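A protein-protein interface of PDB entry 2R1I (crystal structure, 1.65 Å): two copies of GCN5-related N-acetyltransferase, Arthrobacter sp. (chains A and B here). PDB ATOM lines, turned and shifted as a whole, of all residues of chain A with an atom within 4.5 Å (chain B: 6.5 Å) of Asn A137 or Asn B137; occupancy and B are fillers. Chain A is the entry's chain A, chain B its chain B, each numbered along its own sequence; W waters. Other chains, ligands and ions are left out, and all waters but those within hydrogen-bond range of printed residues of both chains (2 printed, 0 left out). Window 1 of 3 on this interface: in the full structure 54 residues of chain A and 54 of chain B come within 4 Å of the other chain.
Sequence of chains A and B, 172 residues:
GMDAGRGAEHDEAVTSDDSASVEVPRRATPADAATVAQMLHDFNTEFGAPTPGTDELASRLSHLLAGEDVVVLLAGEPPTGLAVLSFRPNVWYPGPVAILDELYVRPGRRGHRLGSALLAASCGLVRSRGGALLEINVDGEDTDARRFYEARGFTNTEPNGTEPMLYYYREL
Ile A136 touches Leu B166, and with the chains exchanged Leu A166 touches Ile B136. Ile A136 touches Tyr B167, and with the chains exchanged Tyr A167 touches Ile B136. Asn A137 touches Leu B166, and with the chains exchanged Leu A166 touches Asn B137. Asn A137 touches Tyr B167, and with the chains exchanged Tyr A167 touches Asn B137. Positions printed for both chains: 136, 137, 138, 139, 166 and 167. Of the 18 pairs that touch across the chains among the printed residues, 12 have their exchanged pair printed and touching as well.
Of chain B, only Asn B137, Leu B166 and Tyr B167 come within 4 Å of Asn A137. Printed residues of chain A within 4 Å of Glu B135: Tyr A167 (2.7 Å). Asn B137 touches just these residues of chain A: Asn A137, Leu A166 and Tyr A167. Of the printed residues of chain A, Tyr B168 touches Ile A136 (2.9 Å) and Val A138 (3.7 Å). The nearest printed residue of chain A that does not touch Asn B137 is Ile A136 (5.9 Å).
Water W2 bridges OD1 of Asn A137 (2.8 Å) and OE1 of Glu B135 (2.9 Å). Water W1 lies within hydrogen-bond range of the side-chain carboxylate (OD1) of Asp A139 (2.9 Å) and the backbone NH (N) of Met B165 (3.4 Å).
The backbone NH (N) of Ile A136 is in hydrogen-bond range of the backbone carbonyl oxygen (O) of Tyr B168. The side-chain amide oxygen of Asn B137 is in hydrogen-bond range of the side-chain amide nitrogen of Asn A137 (3.0 Å). The backbone carbonyl oxygen (O) of Val A138 lies within hydrogen-bond range of the backbone NH (N) of Leu B166 (2.8 Å). The backbone NH (N) of Leu A166 sits at hydrogen-bond distance from the backbone carbonyl oxygen (O) of Val B138 (2.8 Å). The side-chain carboxylate (OE2) of Glu B135 is in hydrogen-bond range of the side-chain hydroxyl (OH) of Tyr A167, at 2.7 Å. The backbone NH (N) of Tyr A167 sits at hydrogen-bond distance from the backbone carbonyl oxygen (O) of Met B165.
Hydrophobic or aromatic side chains of chain B that line the printed part of chain A: Met B165, Leu B166, Tyr B167 and Tyr B168.
The guanidinium group of Arg B88 is in salt-bridge range of the side-chain carboxylate of Glu B135 (2.9 Å). The backbone carbonyl oxygen (O) of Glu B135 is in hydrogen-bond range of the backbone NH (N) of Leu B100, 2.8 Å away.
Ile A136 touches Leu B166 (O to O, 3.8 Å). O of Ile A136 touches CA of Tyr B167, 3.6 Å away. Tyr B167 touches Asn A137. Val A138 touches Met B165. Val A138 touches Tyr B168. O of Ile B136 touches O of Leu A166, 3.7 Å away. Leu A166 touches Asn B137 (O to CA, 3.3 Å). Leu A166 touches Met B165 (CA to O, 3.5 Å). CD2 of Leu B166 touches CD2 of Leu A166 (3.9 Å). Tyr A167 touches Asn B137.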
ATOM      1  N   ILE A 136     -11.308   1.714  16.552  1.00  0.00           N
ATOM      2  CA  ILE A 136     -10.855   0.784  15.529  1.00  0.00           C
ATOM      3  C   ILE A 136     -12.069   0.091  14.959  1.00  0.00           C
ATOM      4  O   ILE A 136     -13.042  -0.166  15.678  1.00  0.00           O
ATOM      5  CB  ILE A 136      -9.956  -0.325  16.070  1.00  0.00           C
ATOM      6  CG1 ILE A 136      -9.056   0.117  17.200  1.00  0.00           C
ATOM      7  CG2 ILE A 136      -9.045  -0.921  14.973  1.00  0.00           C
ATOM      8  CD1 ILE A 136      -8.352  -1.119  17.852  1.00  0.00           C
ATOM      9  N   ASN A 137     -11.995  -0.243  13.673  1.00  0.00           N
ATOM     10  CA  ASN A 137     -12.963  -1.121  13.067  1.00  0.00           C
ATOM     11  C   ASN A 137     -12.230  -2.443  12.730  1.00  0.00           C
ATOM     12  O   ASN A 137     -11.157  -2.404  12.122  1.00  0.00           O
ATOM     13  CB  ASN A 137     -13.634  -0.406  11.893  1.00  0.00           C
ATOM     14  CG  ASN A 137     -14.321   0.920  12.346  1.00  0.00           C
ATOM     15  OD1 ASN A 137     -13.904   2.026  11.948  1.00  0.00           O
ATOM     16  ND2 ASN A 137     -15.353   0.807  13.204  1.00  0.00           N
ATOM     17  N   VAL A 138     -12.795  -3.551  13.169  1.00  0.00           N
ATOM     18  CA  VAL A 138     -12.146  -4.874  13.109  1.00  0.00           C
ATOM     19  C   VAL A 138     -13.099  -5.923  12.508  1.00  0.00           C
ATOM     20  O   VAL A 138     -14.269  -6.001  12.890  1.00  0.00           O
ATOM     21  CB  VAL A 138     -11.736  -5.374  14.527  1.00  0.00           C
ATOM     22  CG1 VAL A 138     -11.021  -6.735  14.463  1.00  0.00           C
ATOM     23  CG2 VAL A 138     -10.887  -4.343  15.266  1.00  0.00           C
ATOM     24  N   ASP A 139     -12.616  -6.722  11.562  1.00  0.00           N
ATOM     25  CA  ASP A 139     -13.450  -7.812  11.013  1.00  0.00           C
ATOM     26  C   ASP A 139     -13.749  -8.815  12.114  1.00  0.00           C
ATOM     27  O   ASP A 139     -12.846  -9.234  12.841  1.00  0.00           O
ATOM     28  CB  ASP A 139     -12.737  -8.486   9.838  1.00  0.00           C
ATOM     29  CG  ASP A 139     -13.615  -9.521   9.117  1.00  0.00           C
ATOM     30  OD1 ASP A 139     -14.303 -10.357   9.769  1.00  0.00           O
ATOM     31  OD2 ASP A 139     -13.618  -9.490   7.866  1.00  0.00           O
ATOM     32  N   LEU A 166     -21.442  -2.318  15.769  1.00  0.00           N
ATOM     33  CA  LEU A 166     -21.200  -2.751  14.435  1.00  0.00           C
ATOM     34  C   LEU A 166     -20.701  -1.605  13.554  1.00  0.00           C
ATOM     35  O   LEU A 166     -21.084  -0.472  13.698  1.00  0.00           O
ATOM     36  CB  LEU A 166     -22.502  -3.292  13.826  1.00  0.00           C
ATOM     37  CG  LEU A 166     -23.169  -4.457  14.598  1.00  0.00           C
ATOM     38  CD1 LEU A 166     -24.395  -4.974  13.875  1.00  0.00           C
ATOM     39  CD2 LEU A 166     -22.157  -5.545  14.773  1.00  0.00           C
ATOM     40  N   TYR A 167     -19.835  -1.950  12.621  1.00  0.00           N
ATOM     41  CA  TYR A 167     -19.368  -1.030  11.609  1.00  0.00           C
ATOM     42  C   TYR A 167     -20.136  -1.280  10.310  1.00  0.00           C
ATOM     43  O   TYR A 167     -20.144  -2.400   9.782  1.00  0.00           O
ATOM     44  CB  TYR A 167     -17.846  -1.220  11.410  1.00  0.00           C
ATOM     45  CG  TYR A 167     -17.270  -0.527  10.181  1.00  0.00           C
ATOM     46  CD1 TYR A 167     -16.933   0.833  10.219  1.00  0.00           C
ATOM     47  CD2 TYR A 167     -17.057  -1.211   9.005  1.00  0.00           C
ATOM     48  CE1 TYR A 167     -16.381   1.488   9.085  1.00  0.00           C
ATOM     49  CE2 TYR A 167     -16.538  -0.577   7.877  1.00  0.00           C
ATOM     50  CZ  TYR A 167     -16.169   0.749   7.914  1.00  0.00           C
ATOM     51  OH  TYR A 167     -15.649   1.347   6.780  1.00  0.00           O
ATOM     52  N   ARG B  88     -12.353  13.057   7.083  1.00  0.00           N
ATOM     53  CA  ARG B  88     -10.922  12.911   7.396  1.00  0.00           C
ATOM     54  C   ARG B  88     -10.202  12.368   6.189  1.00  0.00           C
ATOM     55  O   ARG B  88     -10.825  11.749   5.326  1.00  0.00           O
ATOM     56  CB  ARG B  88     -10.740  11.907   8.576  1.00  0.00           C
ATOM     57  CG  ARG B  88     -11.118  10.469   8.219  1.00  0.00           C
ATOM     58  CD  ARG B  88     -11.222   9.592   9.481  1.00  0.00           C
ATOM     59  NE  ARG B  88     -11.217   8.194   9.096  1.00  0.00           N
ATOM     60  CZ  ARG B  88     -12.300   7.460   8.845  1.00  0.00           C
ATOM     61  NH1 ARG B  88     -13.495   7.995   8.891  1.00  0.00           N
ATOM     62  NH2 ARG B  88     -12.182   6.196   8.473  1.00  0.00           N
ATOM     63  N   ILE B  99     -17.885   9.951   8.116  1.00  0.00           N
ATOM     64  CA  ILE B  99     -18.693   9.173   9.067  1.00  0.00           C
ATOM     65  C   ILE B  99     -19.975   9.946   9.307  1.00  0.00           C
ATOM     66  O   ILE B  99     -19.916  11.173   9.456  1.00  0.00           O
ATOM     67  CB  ILE B  99     -17.959   8.993  10.426  1.00  0.00           C
ATOM     68  CG1 ILE B  99     -16.646   8.242  10.180  1.00  0.00           C
ATOM     69  CG2 ILE B  99     -18.839   8.222  11.414  1.00  0.00           C
ATOM     70  CD1 ILE B  99     -15.683   8.405  11.439  1.00  0.00           C
ATOM     71  N   LEU B 100     -21.088   9.216   9.316  1.00  0.00           N
ATOM     72  CA  LEU B 100     -22.339   9.744   9.857  1.00  0.00           C
ATOM     73  C   LEU B 100     -22.242   9.624  11.374  1.00  0.00           C
ATOM     74  O   LEU B 100     -22.527   8.572  11.987  1.00  0.00           O
ATOM     75  CB  LEU B 100     -23.543   8.952   9.304  1.00  0.00           C
ATOM     76  CG  LEU B 100     -24.934   9.422   9.683  1.00  0.00           C
ATOM     77  CD1 LEU B 100     -25.143  10.822   9.128  1.00  0.00           C
ATOM     78  CD2 LEU B 100     -25.947   8.385   9.116  1.00  0.00           C
ATOM     79  N   ASP B 101     -21.701  10.673  11.970  1.00  0.00           N
ATOM     80  CA  ASP B 101     -21.482  10.753  13.397  1.00  0.00           C
ATOM     81  C   ASP B 101     -22.810  10.634  14.160  1.00  0.00           C
ATOM     82  O   ASP B 101     -22.853   9.961  15.208  1.00  0.00           O
ATOM     83  CB  ASP B 101     -20.861  12.097  13.775  1.00  0.00           C
ATOM     84  CG  ASP B 101     -19.414  12.272  13.397  1.00  0.00           C
ATOM     85  OD1 ASP B 101     -18.807  11.379  12.747  1.00  0.00           O
ATOM     86  OD2 ASP B 101     -18.873  13.400  13.729  1.00  0.00           O
ATOM     87  N   GLU B 135     -19.227   5.845   6.403  1.00  0.00           N
ATOM     88  CA  GLU B 135     -19.181   4.895   7.502  1.00  0.00           C
ATOM     89  C   GLU B 135     -20.192   5.296   8.628  1.00  0.00           C
ATOM     90  O   GLU B 135     -20.472   6.484   8.853  1.00  0.00           O
ATOM     91  CB  GLU B 135     -17.772   4.922   8.097  1.00  0.00           C
ATOM     92  CG  GLU B 135     -16.691   4.592   7.077  1.00  0.00           C
ATOM     93  CD  GLU B 135     -15.301   4.564   7.693  1.00  0.00           C
ATOM     94  OE1 GLU B 135     -15.000   5.435   8.573  1.00  0.00           O
ATOM     95  OE2 GLU B 135     -14.506   3.708   7.262  1.00  0.00           O
ATOM     96  N   ILE B 136     -20.660   4.295   9.369  1.00  0.00           N
ATOM     97  CA  ILE B 136     -21.509   4.467  10.537  1.00  0.00           C
ATOM     98  C   ILE B 136     -21.101   3.424  11.565  1.00  0.00           C
ATOM     99  O   ILE B 136     -20.732   2.284  11.212  1.00  0.00           O
ATOM    100  CB  ILE B 136     -23.028   4.271  10.216  1.00  0.00           C
ATOM    101  CG1 ILE B 136     -23.441   4.800   8.851  1.00  0.00           C
ATOM    102  CG2 ILE B 136     -23.891   4.956  11.335  1.00  0.00           C
ATOM    103  CD1 ILE B 136     -24.945   4.457   8.493  1.00  0.00           C
ATOM    104  N   ASN B 137     -21.129   3.801  12.826  1.00  0.00           N
ATOM    105  CA  ASN B 137     -21.018   2.825  13.925  1.00  0.00           C
ATOM    106  C   ASN B 137     -22.419   2.701  14.578  1.00  0.00           C
ATOM    107  O   ASN B 137     -23.006   3.706  14.918  1.00  0.00           O
ATOM    108  CB  ASN B 137     -19.854   3.225  14.848  1.00  0.00           C
ATOM    109  CG  ASN B 137     -18.461   3.234  14.071  1.00  0.00           C
ATOM    110  OD1 ASN B 137     -18.021   2.217  13.507  1.00  0.00           O
ATOM    111  ND2 ASN B 137     -17.807   4.414  14.020  1.00  0.00           N
ATOM    112  N   VAL B 138     -22.958   1.491  14.643  1.00  0.00           N
ATOM    113  CA  VAL B 138     -24.346   1.278  15.033  1.00  0.00           C
ATOM    114  C   VAL B 138     -24.384   0.206  16.162  1.00  0.00           C
ATOM    115  O   VAL B 138     -23.763  -0.827  16.061  1.00  0.00           O
ATOM    116  CB  VAL B 138     -25.216   0.828  13.817  1.00  0.00           C
ATOM    117  CG1 VAL B 138     -26.684   0.563  14.222  1.00  0.00           C
ATOM    118  CG2 VAL B 138     -25.169   1.884  12.628  1.00  0.00           C
ATOM    119  N   ASP B 139     -25.101   0.503  17.239  1.00  0.00           N
ATOM    120  CA  ASP B 139     -25.371  -0.498  18.304  1.00  0.00           C
ATOM    121  C   ASP B 139     -26.061  -1.706  17.674  1.00  0.00           C
ATOM    122  O   ASP B 139     -27.105  -1.564  17.019  1.00  0.00           O
ATOM    123  CB  ASP B 139     -26.247   0.146  19.383  1.00  0.00           C
ATOM    124  CG  ASP B 139     -26.456  -0.735  20.619  1.00  0.00           C
ATOM    125  OD1 ASP B 139     -26.064  -1.922  20.666  1.00  0.00           O
ATOM    126  OD2 ASP B 139     -27.073  -0.214  21.568  1.00  0.00           O
ATOM    127  N   MET B 165     -18.654  -6.712  10.830  1.00  0.00           N
ATOM    128  CA  MET B 165     -17.526  -5.873  11.162  1.00  0.00           C
ATOM    129  C   MET B 165     -17.865  -5.200  12.470  1.00  0.00           C
ATOM    130  O   MET B 165     -19.028  -4.855  12.748  1.00  0.00           O
ATOM    131  CB  MET B 165     -17.328  -4.846  10.074  1.00  0.00           C
ATOM    132  CG  MET B 165     -17.708  -5.410   8.729  1.00  0.00           C
ATOM    133  SD  MET B 165     -16.620  -4.684   7.408  1.00  0.00           S
ATOM    134  CE  MET B 165     -14.970  -5.351   8.244  1.00  0.00           C
ATOM    135  N   LEU B 166     -16.855  -5.046  13.304  1.00  0.00           N
ATOM    136  CA  LEU B 166     -17.091  -4.537  14.650  1.00  0.00           C
ATOM    137  C   LEU B 166     -16.388  -3.224  14.949  1.00  0.00           C
ATOM    138  O   LEU B 166     -15.295  -2.970  14.455  1.00  0.00           O
ATOM    139  CB  LEU B 166     -16.587  -5.572  15.657  1.00  0.00           C
ATOM    140  CG  LEU B 166     -17.161  -7.007  15.522  1.00  0.00           C
ATOM    141  CD1 LEU B 166     -16.546  -7.932  16.572  1.00  0.00           C
ATOM    142  CD2 LEU B 166     -18.668  -6.962  15.639  1.00  0.00           C
ATOM    143  N   TYR B 167     -17.049  -2.386  15.762  1.00  0.00           N
ATOM    144  CA  TYR B 167     -16.462  -1.173  16.298  1.00  0.00           C
ATOM    145  C   TYR B 167     -15.907  -1.414  17.712  1.00  0.00           C
ATOM    146  O   TYR B 167     -16.603  -1.939  18.584  1.00  0.00           O
ATOM    147  CB  TYR B 167     -17.530  -0.084  16.307  1.00  0.00           C
ATOM    148  CG  TYR B 167     -17.167   1.178  17.061  1.00  0.00           C
ATOM    149  CD1 TYR B 167     -17.485   1.314  18.408  1.00  0.00           C
ATOM    150  CD2 TYR B 167     -16.540   2.231  16.424  1.00  0.00           C
ATOM    151  CE1 TYR B 167     -17.184   2.490  19.115  1.00  0.00           C
ATOM    152  CE2 TYR B 167     -16.249   3.397  17.115  1.00  0.00           C
ATOM    153  CZ  TYR B 167     -16.574   3.537  18.451  1.00  0.00           C
ATOM    154  OH  TYR B 167     -16.262   4.697  19.141  1.00  0.00           O
ATOM    155  N   TYR B 168     -14.625  -1.089  17.888  1.00  0.00           N
ATOM    156  CA  TYR B 168     -13.898  -1.116  19.156  1.00  0.00           C
ATOM    157  C   TYR B 168     -13.436   0.294  19.556  1.00  0.00           C
ATOM    158  O   TYR B 168     -13.125   1.152  18.694  1.00  0.00           O
ATOM    159  CB  TYR B 168     -12.659  -2.033  19.035  1.00  0.00           C
ATOM    160  CG  TYR B 168     -12.946  -3.509  19.159  1.00  0.00           C
ATOM    161  CD1 TYR B 168     -13.341  -4.264  18.037  1.00  0.00           C
ATOM    162  CD2 TYR B 168     -12.752  -4.175  20.354  1.00  0.00           C
ATOM    163  CE1 TYR B 168     -13.613  -5.655  18.143  1.00  0.00           C
ATOM    164  CE2 TYR B 168     -12.990  -5.544  20.457  1.00  0.00           C
ATOM    165  CZ  TYR B 168     -13.403  -6.277  19.340  1.00  0.00           C
ATOM    166  OH  TYR B 168     -13.676  -7.624  19.489  1.00  0.00           O
HETATM  167  O   HOH W   1     -16.396  -8.546   9.086  1.00  0.00           O
HETATM  168  O   HOH W   2     -15.153   4.508  11.339  1.00  0.00           O
